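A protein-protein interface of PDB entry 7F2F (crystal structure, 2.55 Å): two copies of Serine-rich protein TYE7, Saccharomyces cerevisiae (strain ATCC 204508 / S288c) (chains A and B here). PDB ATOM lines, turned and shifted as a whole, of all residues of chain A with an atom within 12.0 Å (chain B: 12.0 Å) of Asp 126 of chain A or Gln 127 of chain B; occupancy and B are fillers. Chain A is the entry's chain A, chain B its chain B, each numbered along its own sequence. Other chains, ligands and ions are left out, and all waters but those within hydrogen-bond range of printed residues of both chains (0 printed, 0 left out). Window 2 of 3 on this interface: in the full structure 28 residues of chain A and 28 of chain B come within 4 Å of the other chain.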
ATOM      1  N   LEU A 116      -6.933  -3.987  30.692  1.00  0.00           N
ATOM      2  CA  LEU A 116      -7.564  -2.682  30.864  1.00  0.00           C
ATOM      3  C   LEU A 116      -6.525  -1.650  31.256  1.00  0.00           C
ATOM      4  O   LEU A 116      -6.471  -0.573  30.673  1.00  0.00           O
ATOM      5  CB  LEU A 116      -8.721  -2.707  31.905  1.00  0.00           C
ATOM      6  CG  LEU A 116      -9.903  -3.582  31.521  1.00  0.00           C
ATOM      7  CD1 LEU A 116     -10.766  -4.014  32.716  1.00  0.00           C
ATOM      8  CD2 LEU A 116     -10.740  -2.971  30.420  1.00  0.00           C
ATOM      9  N   LYS A 117      -5.714  -1.972  32.252  1.00  0.00           N
ATOM     10  CA  LYS A 117      -4.619  -1.099  32.629  1.00  0.00           C
ATOM     11  C   LYS A 117      -3.770  -0.702  31.429  1.00  0.00           C
ATOM     12  O   LYS A 117      -3.475   0.477  31.254  1.00  0.00           O
ATOM     13  CB  LYS A 117      -3.779  -1.703  33.748  1.00  0.00           C
ATOM     14  CG  LYS A 117      -4.563  -1.727  35.068  1.00  0.00           C
ATOM     15  CD  LYS A 117      -3.719  -1.947  36.298  1.00  0.00           C
ATOM     16  CE  LYS A 117      -4.586  -1.839  37.538  1.00  0.00           C
ATOM     17  NZ  LYS A 117      -3.963  -2.406  38.765  1.00  0.00           N
ATOM     18  N   SER A 118      -3.478  -1.642  30.547  1.00  0.00           N
ATOM     19  CA  SER A 118      -2.677  -1.321  29.402  1.00  0.00           C
ATOM     20  C   SER A 118      -3.449  -0.506  28.340  1.00  0.00           C
ATOM     21  O   SER A 118      -2.886   0.372  27.723  1.00  0.00           O
ATOM     22  CB  SER A 118      -1.966  -2.573  28.852  1.00  0.00           C
ATOM     23  OG  SER A 118      -2.779  -3.275  27.978  1.00  0.00           O
ATOM     24  N   GLU A 119      -4.735  -0.742  28.164  1.00  0.00           N
ATOM     25  CA  GLU A 119      -5.537   0.158  27.339  1.00  0.00           C
ATOM     26  C   GLU A 119      -5.514   1.581  27.885  1.00  0.00           C
ATOM     27  O   GLU A 119      -5.421   2.527  27.093  1.00  0.00           O
ATOM     28  CB  GLU A 119      -6.967  -0.328  27.147  1.00  0.00           C
ATOM     29  CG  GLU A 119      -7.881   0.696  26.502  1.00  0.00           C
ATOM     30  CD  GLU A 119      -9.110   0.099  25.813  1.00  0.00           C
ATOM     31  OE1 GLU A 119      -9.525  -1.014  26.233  1.00  0.00           O
ATOM     32  OE2 GLU A 119      -9.654   0.766  24.852  1.00  0.00           O
ATOM     33  N   ILE A 120      -5.549   1.745  29.204  1.00  0.00           N
ATOM     34  CA  ILE A 120      -5.333   3.082  29.817  1.00  0.00           C
ATOM     35  C   ILE A 120      -3.936   3.639  29.556  1.00  0.00           C
ATOM     36  O   ILE A 120      -3.819   4.767  29.104  1.00  0.00           O
ATOM     37  CB  ILE A 120      -5.560   3.083  31.337  1.00  0.00           C
ATOM     38  CG1 ILE A 120      -7.037   2.970  31.663  1.00  0.00           C
ATOM     39  CG2 ILE A 120      -5.006   4.330  31.995  1.00  0.00           C
ATOM     40  CD1 ILE A 120      -7.257   2.388  33.053  1.00  0.00           C
ATOM     41  N   ASP A 121      -2.893   2.868  29.866  1.00  0.00           N
ATOM     42  CA  ASP A 121      -1.519   3.261  29.521  1.00  0.00           C
ATOM     43  C   ASP A 121      -1.578   3.890  28.148  1.00  0.00           C
ATOM     44  O   ASP A 121      -1.197   5.040  27.993  1.00  0.00           O
ATOM     45  CB  ASP A 121      -0.512   2.078  29.418  1.00  0.00           C
ATOM     46  CG  ASP A 121      -0.274   1.334  30.740  1.00  0.00           C
ATOM     47  OD1 ASP A 121      -0.656   1.861  31.812  1.00  0.00           O
ATOM     48  OD2 ASP A 121       0.295   0.204  30.688  1.00  0.00           O
ATOM     49  N   THR A 122      -2.077   3.129  27.166  1.00  0.00           N
ATOM     50  CA  THR A 122      -1.964   3.515  25.783  1.00  0.00           C
ATOM     51  C   THR A 122      -2.822   4.716  25.343  1.00  0.00           C
ATOM     52  O   THR A 122      -2.538   5.312  24.320  1.00  0.00           O
ATOM     53  CB  THR A 122      -2.116   2.316  24.841  1.00  0.00           C
ATOM     54  OG1 THR A 122      -1.736   2.710  23.525  1.00  0.00           O
ATOM     55  CG2 THR A 122      -3.524   1.816  24.766  1.00  0.00           C
ATOM     56  N   LEU A 123      -3.855   5.075  26.104  1.00  0.00           N
ATOM     57  CA  LEU A 123      -4.596   6.322  25.866  1.00  0.00           C
ATOM     58  C   LEU A 123      -3.866   7.503  26.465  1.00  0.00           C
ATOM     59  O   LEU A 123      -3.746   8.522  25.807  1.00  0.00           O
ATOM     60  CB  LEU A 123      -6.011   6.273  26.447  1.00  0.00           C
ATOM     61  CG  LEU A 123      -6.990   5.362  25.712  1.00  0.00           C
ATOM     62  CD1 LEU A 123      -8.159   5.042  26.616  1.00  0.00           C
ATOM     63  CD2 LEU A 123      -7.469   5.950  24.399  1.00  0.00           C
ATOM     64  N   LYS A 124      -3.415   7.376  27.711  1.00  0.00           N
ATOM     65  CA  LYS A 124      -2.631   8.432  28.412  1.00  0.00           C
ATOM     66  C   LYS A 124      -1.272   8.877  27.801  1.00  0.00           C
ATOM     67  O   LYS A 124      -0.860  10.017  28.040  1.00  0.00           O
ATOM     68  CB  LYS A 124      -2.326   8.020  29.858  1.00  0.00           C
ATOM     69  CG  LYS A 124      -3.459   8.173  30.859  1.00  0.00           C
ATOM     70  CD  LYS A 124      -2.889   8.300  32.272  1.00  0.00           C
ATOM     71  CE  LYS A 124      -3.701   7.568  33.325  1.00  0.00           C
ATOM     72  NZ  LYS A 124      -5.045   8.167  33.529  1.00  0.00           N
ATOM     73  N   GLN A 125      -0.559   7.995  27.085  1.00  0.00           N
ATOM     74  CA  GLN A 125       0.720   8.367  26.420  1.00  0.00           C
ATOM     75  C   GLN A 125       0.493   9.270  25.195  1.00  0.00           C
ATOM     76  O   GLN A 125       1.411   9.956  24.739  1.00  0.00           O
ATOM     77  CB  GLN A 125       1.555   7.140  26.026  1.00  0.00           C
ATOM     78  CG  GLN A 125       0.958   6.278  24.912  1.00  0.00           C
ATOM     79  CD  GLN A 125       1.884   5.164  24.451  1.00  0.00           C
ATOM     80  OE1 GLN A 125       2.590   4.539  25.246  1.00  0.00           O
ATOM     81  NE2 GLN A 125       1.875   4.906  23.153  1.00  0.00           N
ATOM     82  N   ASP A 126      -0.729   9.244  24.658  1.00  0.00           N
ATOM     83  CA  ASP A 126      -1.183  10.260  23.702  1.00  0.00           C
ATOM     84  C   ASP A 126      -1.177  11.631  24.397  1.00  0.00           C
ATOM     85  O   ASP A 126      -0.554  12.573  23.911  1.00  0.00           O
ATOM     86  CB  ASP A 126      -2.608   9.960  23.171  1.00  0.00           C
ATOM     87  CG  ASP A 126      -2.786   8.512  22.672  1.00  0.00           C
ATOM     88  OD1 ASP A 126      -1.785   7.875  22.260  1.00  0.00           O
ATOM     89  OD2 ASP A 126      -3.941   8.017  22.695  1.00  0.00           O
ATOM     90  N   GLN A 127      -1.833  11.681  25.561  1.00  0.00           N
ATOM     91  CA  GLN A 127      -2.216  12.901  26.274  1.00  0.00           C
ATOM     92  C   GLN A 127      -3.132  13.740  25.380  1.00  0.00           C
ATOM     93  O   GLN A 127      -4.026  13.192  24.719  1.00  0.00           O
ATOM     94  CB  GLN A 127      -1.012  13.687  26.870  1.00  0.00           C
ATOM     95  CG  GLN A 127      -0.170  14.575  25.932  1.00  0.00           C
ATOM     96  CD  GLN A 127       0.472  15.791  26.615  1.00  0.00           C
ATOM     97  OE1 GLN A 127       0.297  16.018  27.809  1.00  0.00           O
ATOM     98  NE2 GLN A 127       1.223  16.582  25.843  1.00  0.00           N
ATOM     99  N   SER B 118     -14.431   2.505  33.612  1.00  0.00           N
ATOM    100  CA  SER B 118     -14.972   3.811  33.792  1.00  0.00           C
ATOM    101  C   SER B 118     -13.931   4.835  33.387  1.00  0.00           C
ATOM    102  O   SER B 118     -14.232   5.709  32.593  1.00  0.00           O
ATOM    103  CB  SER B 118     -15.419   4.001  35.239  1.00  0.00           C
ATOM    104  OG  SER B 118     -15.812   5.316  35.467  1.00  0.00           O
ATOM    105  N   GLU B 119     -12.715   4.694  33.919  1.00  0.00           N
ATOM    106  CA  GLU B 119     -11.552   5.532  33.577  1.00  0.00           C
ATOM    107  C   GLU B 119     -11.239   5.521  32.065  1.00  0.00           C
ATOM    108  O   GLU B 119     -10.901   6.539  31.498  1.00  0.00           O
ATOM    109  CB  GLU B 119     -10.362   5.116  34.428  1.00  0.00           C
ATOM    110  CG  GLU B 119      -9.061   5.825  34.112  1.00  0.00           C
ATOM    111  CD  GLU B 119      -7.993   5.709  35.234  1.00  0.00           C
ATOM    112  OE1 GLU B 119      -8.121   4.837  36.159  1.00  0.00           O
ATOM    113  OE2 GLU B 119      -7.004   6.507  35.182  1.00  0.00           O
ATOM    114  N   ILE B 120     -11.443   4.398  31.395  1.00  0.00           N
ATOM    115  CA  ILE B 120     -11.263   4.328  29.934  1.00  0.00           C
ATOM    116  C   ILE B 120     -12.313   5.121  29.240  1.00  0.00           C
ATOM    117  O   ILE B 120     -12.038   5.799  28.271  1.00  0.00           O
ATOM    118  CB  ILE B 120     -11.244   2.866  29.421  1.00  0.00           C
ATOM    119  CG1 ILE B 120      -9.841   2.289  29.698  1.00  0.00           C
ATOM    120  CG2 ILE B 120     -11.654   2.725  27.954  1.00  0.00           C
ATOM    121  CD1 ILE B 120      -9.822   0.795  30.031  1.00  0.00           C
ATOM    122  N   ASP B 121     -13.517   5.027  29.734  1.00  0.00           N
ATOM    123  CA  ASP B 121     -14.574   5.825  29.201  1.00  0.00           C
ATOM    124  C   ASP B 121     -14.288   7.304  29.314  1.00  0.00           C
ATOM    125  O   ASP B 121     -14.373   8.019  28.325  1.00  0.00           O
ATOM    126  CB  ASP B 121     -15.852   5.535  29.938  1.00  0.00           C
ATOM    127  CG  ASP B 121     -16.978   6.253  29.347  1.00  0.00           C
ATOM    128  OD1 ASP B 121     -17.298   5.905  28.195  1.00  0.00           O
ATOM    129  OD2 ASP B 121     -17.478   7.188  30.013  1.00  0.00           O
ATOM    130  N   THR B 122     -13.858   7.755  30.495  1.00  0.00           N
ATOM    131  CA  THR B 122     -13.703   9.180  30.664  1.00  0.00           C
ATOM    132  C   THR B 122     -12.552   9.664  29.774  1.00  0.00           C
ATOM    133  O   THR B 122     -12.702  10.701  29.158  1.00  0.00           O
ATOM    134  CB  THR B 122     -13.692   9.725  32.138  1.00  0.00           C
ATOM    135  OG1 THR B 122     -12.410  10.203  32.490  1.00  0.00           O
ATOM    136  CG2 THR B 122     -14.227   8.746  33.205  1.00  0.00           C
ATOM    137  N   LEU B 123     -11.464   8.887  29.618  1.00  0.00           N
ATOM    138  CA  LEU B 123     -10.387   9.271  28.685  1.00  0.00           C
ATOM    139  C   LEU B 123     -10.845   9.338  27.251  1.00  0.00           C
ATOM    140  O   LEU B 123     -10.399  10.226  26.492  1.00  0.00           O
ATOM    141  CB  LEU B 123      -9.215   8.316  28.701  1.00  0.00           C
ATOM    142  CG  LEU B 123      -8.317   8.315  29.927  1.00  0.00           C
ATOM    143  CD1 LEU B 123      -7.499   7.025  29.905  1.00  0.00           C
ATOM    144  CD2 LEU B 123      -7.421   9.544  30.005  1.00  0.00           C
ATOM    145  N   LYS B 124     -11.697   8.407  26.848  1.00  0.00           N
ATOM    146  CA  LYS B 124     -12.133   8.440  25.469  1.00  0.00           C
ATOM    147  C   LYS B 124     -13.040   9.633  25.222  1.00  0.00           C
ATOM    148  O   LYS B 124     -12.964  10.235  24.157  1.00  0.00           O
ATOM    149  CB  LYS B 124     -12.796   7.149  25.043  1.00  0.00           C
ATOM    150  CG  LYS B 124     -11.788   6.035  24.866  1.00  0.00           C
ATOM    151  CD  LYS B 124     -12.463   4.751  24.398  1.00  0.00           C
ATOM    152  CE  LYS B 124     -11.469   3.793  23.766  1.00  0.00           C
ATOM    153  NZ  LYS B 124     -12.123   2.489  23.495  1.00  0.00           N
ATOM    154  N   GLN B 125     -13.855  10.002  26.199  1.00  0.00           N
ATOM    155  CA  GLN B 125     -14.684  11.198  26.047  1.00  0.00           C
ATOM    156  C   GLN B 125     -13.849  12.479  25.947  1.00  0.00           C
ATOM    157  O   GLN B 125     -13.852  13.163  24.912  1.00  0.00           O
ATOM    158  CB  GLN B 125     -15.701  11.306  27.186  1.00  0.00           C
ATOM    159  CG  GLN B 125     -16.786  10.262  27.125  1.00  0.00           C
ATOM    160  CD  GLN B 125     -17.435  10.259  25.767  1.00  0.00           C
ATOM    161  OE1 GLN B 125     -17.044   9.479  24.910  1.00  0.00           O
ATOM    162  NE2 GLN B 125     -18.371  11.200  25.532  1.00  0.00           N
ATOM    163  N   ASP B 126     -13.107  12.770  27.006  1.00  0.00           N
ATOM    164  CA  ASP B 126     -12.176  13.901  27.028  1.00  0.00           C
ATOM    165  C   ASP B 126     -11.431  14.045  25.696  1.00  0.00           C
ATOM    166  O   ASP B 126     -11.338  15.144  25.159  1.00  0.00           O
ATOM    167  CB  ASP B 126     -11.138  13.749  28.149  1.00  0.00           C
ATOM    168  CG  ASP B 126     -11.743  13.857  29.556  1.00  0.00           C
ATOM    169  OD1 ASP B 126     -13.003  13.974  29.724  1.00  0.00           O
ATOM    170  OD2 ASP B 126     -10.926  13.798  30.509  1.00  0.00           O
ATOM    171  N   GLN B 127     -10.923  12.934  25.169  1.00  0.00           N
ATOM    172  CA  GLN B 127     -10.192  12.964  23.917  1.00  0.00           C
ATOM    173  C   GLN B 127     -11.070  13.204  22.706  1.00  0.00           C
ATOM    174  O   GLN B 127     -10.673  13.915  21.798  1.00  0.00           O
ATOM    175  CB  GLN B 127      -9.396  11.685  23.710  1.00  0.00           C
ATOM    176  CG  GLN B 127      -8.140  11.632  24.541  1.00  0.00           C
ATOM    177  CD  GLN B 127      -7.300  10.401  24.257  1.00  0.00           C
ATOM    178  OE1 GLN B 127      -6.514   9.986  25.108  1.00  0.00           O
ATOM    179  NE2 GLN B 127      -7.460   9.801  23.059  1.00  0.00           N
ATOM    180  N   LYS B 128     -12.252  12.608  22.687  1.00  0.00           N
ATOM    181  CA  LYS B 128     -13.178  12.796  21.579  1.00  0.00           C
ATOM    182  C   LYS B 128     -13.706  14.237  21.543  1.00  0.00           C
ATOM    183  O   LYS B 128     -13.797  14.805  20.482  1.00  0.00           O
ATOM    184  CB  LYS B 128     -14.323  11.836  21.747  1.00  0.00           C
ATOM    185  CG  LYS B 128     -15.287  11.757  20.608  1.00  0.00           C
ATOM    186  CD  LYS B 128     -16.553  11.038  21.056  1.00  0.00           C
ATOM    187  CE  LYS B 128     -16.387   9.536  21.236  1.00  0.00           C
ATOM    188  NZ  LYS B 128     -15.883   8.921  19.972  1.00  0.00           N
ATOM    189  N   LEU B 129     -14.031  14.817  22.697  1.00  0.00           N
ATOM    190  CA  LEU B 129     -14.578  16.173  22.767  1.00  0.00           C
ATOM    191  C   LEU B 129     -13.587  17.339  22.975  1.00  0.00           C
ATOM    192  O   LEU B 129     -14.031  18.478  23.027  1.00  0.00           O
ATOM    193  CB  LEU B 129     -15.667  16.252  23.840  1.00  0.00           C
ATOM    194  CG  LEU B 129     -16.753  15.198  23.650  1.00  0.00           C
ATOM    195  CD1 LEU B 129     -17.829  15.290  24.702  1.00  0.00           C
ATOM    196  CD2 LEU B 129     -17.361  15.211  22.252  1.00  0.00           C
ATOM    197  N   GLU B 130     -12.274  17.106  23.063  1.00  0.00           N
ATOM    198  CA  GLU B 130     -11.332  18.243  23.270  1.00  0.00           C
ATOM    199  C   GLU B 130     -11.400  19.301  22.132  1.00  0.00           C
ATOM    200  O   GLU B 130     -11.593  20.488  22.403  1.00  0.00           O
ATOM    201  CB  GLU B 130      -9.886  17.771  23.520  1.00  0.00           C
ATOM    202  CG  GLU B 130      -9.159  17.153  22.330  1.00  0.00           C
ATOM    203  CD  GLU B 130      -7.793  16.607  22.707  1.00  0.00           C
ATOM    204  OE1 GLU B 130      -7.707  15.724  23.591  1.00  0.00           O
ATOM    205  OE2 GLU B 130      -6.791  17.057  22.116  1.00  0.00           O
ATOM    206  N   HIS B 131     -11.306  18.839  20.883  1.00  0.00           N
ATOM    207  CA  HIS B 131     -11.377  19.687  19.685  1.00  0.00           C
ATOM    208  C   HIS B 131     -12.716  20.483  19.627  1.00  0.00           C
ATOM    209  O   HIS B 131     -12.753  21.611  19.155  1.00  0.00           O
ATOM    210  CB  HIS B 131     -11.205  18.793  18.436  1.00  0.00           C
ATOM    211  CG  HIS B 131     -10.519  19.454  17.279  1.00  0.00           C
ATOM    212  ND1 HIS B 131      -9.277  20.047  17.383  1.00  0.00           N
ATOM    213  CD2 HIS B 131     -10.877  19.561  15.975  1.00  0.00           C
ATOM    214  CE1 HIS B 131      -8.916  20.520  16.203  1.00  0.00           C
ATOM    215  NE2 HIS B 131      -9.868  20.237  15.332  1.00  0.00           N
ATOM    216  N   HIS B 132     -13.796  19.868  20.111  1.00  0.00           N
ATOM    217  CA  HIS B 132     -15.139  20.469  20.225  1.00  0.00           C
ATOM    218  C   HIS B 132     -15.110  21.453  21.392  1.00  0.00           C
ATOM    219  O   HIS B 132     -16.139  21.959  21.832  1.00  0.00           O
ATOM    220  CB  HIS B 132     -16.151  19.318  20.463  1.00  0.00           C
ATOM    221  CG  HIS B 132     -17.601  19.708  20.486  1.00  0.00           C
ATOM    222  ND1 HIS B 132     -18.380  19.583  21.622  1.00  0.00           N
ATOM    223  CD2 HIS B 132     -18.437  20.126  19.505  1.00  0.00           C
ATOM    224  CE1 HIS B 132     -19.623  19.942  21.349  1.00  0.00           C
ATOM    225  NE2 HIS B 132     -19.686  20.278  20.071  1.00  0.00           N
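The side-chain amide oxygen of Gln 127 of chain B sits close to the backbone carbonyl oxygen of Leu 123 of chain A (3.2 Å). The side-chain carboxylate of Glu 119 of chain B lies within salt-bridge range of the side-chain amino group of Lys 124 of chain A (3.1 Å). The side-chain carboxylate (OE2) of Glu 119 of chain A is in salt-bridge range of the side-chain amino group (NZ) of Lys 124 of chain B.
CD1 of Ile 120 of chain B touches O of Leu 116 of chain A, at 3.7 Å. Ile 120 of chain A touches Ile 120 of chain B. Leu 123 of chain B touches Leu 123 of chain A. Asp 126 of chain A touches Gln 127 of chain B (OD2 to NE2, 3.96 Å).
Of chain B, only Gln 127 comes within 4 Å of Asp 126 of chain A. Of the printed residues of chain A, Gln 127 of chain B touches Leu 123 and Asp 126. No residue of chain B comes within 4 Å of Thr 122 of chain A. No residue of chain B comes within 4 Å of Gln 125 of chain A. Of chain A, only Leu 123 (3.8 Å) comes within 4 Å of Leu 123 of chain B. No residue of chain A comes within 4 Å of Gln 125 of chain B. No residue of chain A comes within 4 Å of Asp 126 of chain B. No residue of chain A comes within 4 Å of Lys 128 of chain B. No residue of chain A comes within 4 Å of Leu 129 of chain B. Of the printed residues of chain B, Glu 119 of chain A touches Lys 124 (3.3 Å). Of the printed residues of chain B, Ile 120 of chain A touches Ile 120. Printed residues of chain B within 4 Å of Leu 116 of chain A: Ile 120. Ser 118 of chain A touches none of the printed residues of chain B. The nearest residue of chain B that does not touch Asp 126 of chain A is Glu 130 of chain B (7.7 Å). The nearest printed residue of chain A that does not touch Glu 119 of chain B is Ile 120 of chain A (4.02 Å).
Among the printed residues, Asp or Glu carboxylates within 4 Å of a Lys or Arg side-chain nitrogen of the other chain: Glu 119 of chain A with Lys 124 of chain B (3.3 Å) and Lys 124 of chain A with Glu 119 of chain B (3.1 Å).
Ile 120 of chain B touches its own counterpart, Ile 120 of chain A. Leu 123 of chain B touches its own counterpart, Leu 123 of chain A. Leu 123 of chain A touches Gln 127 of chain B, but with the chains exchanged Gln 127 of chain A does not touch Leu 123 of chain B (7.2 Å). Asp 126 of chain A touches Gln 127 of chain B, but with the chains exchanged Gln 127 of chain A does not touch Asp 126 of chain B (7.5 Å). Positions printed for both chains: 118, 119, 120, 121, 122, 123, 124, 125, 126 and 127.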
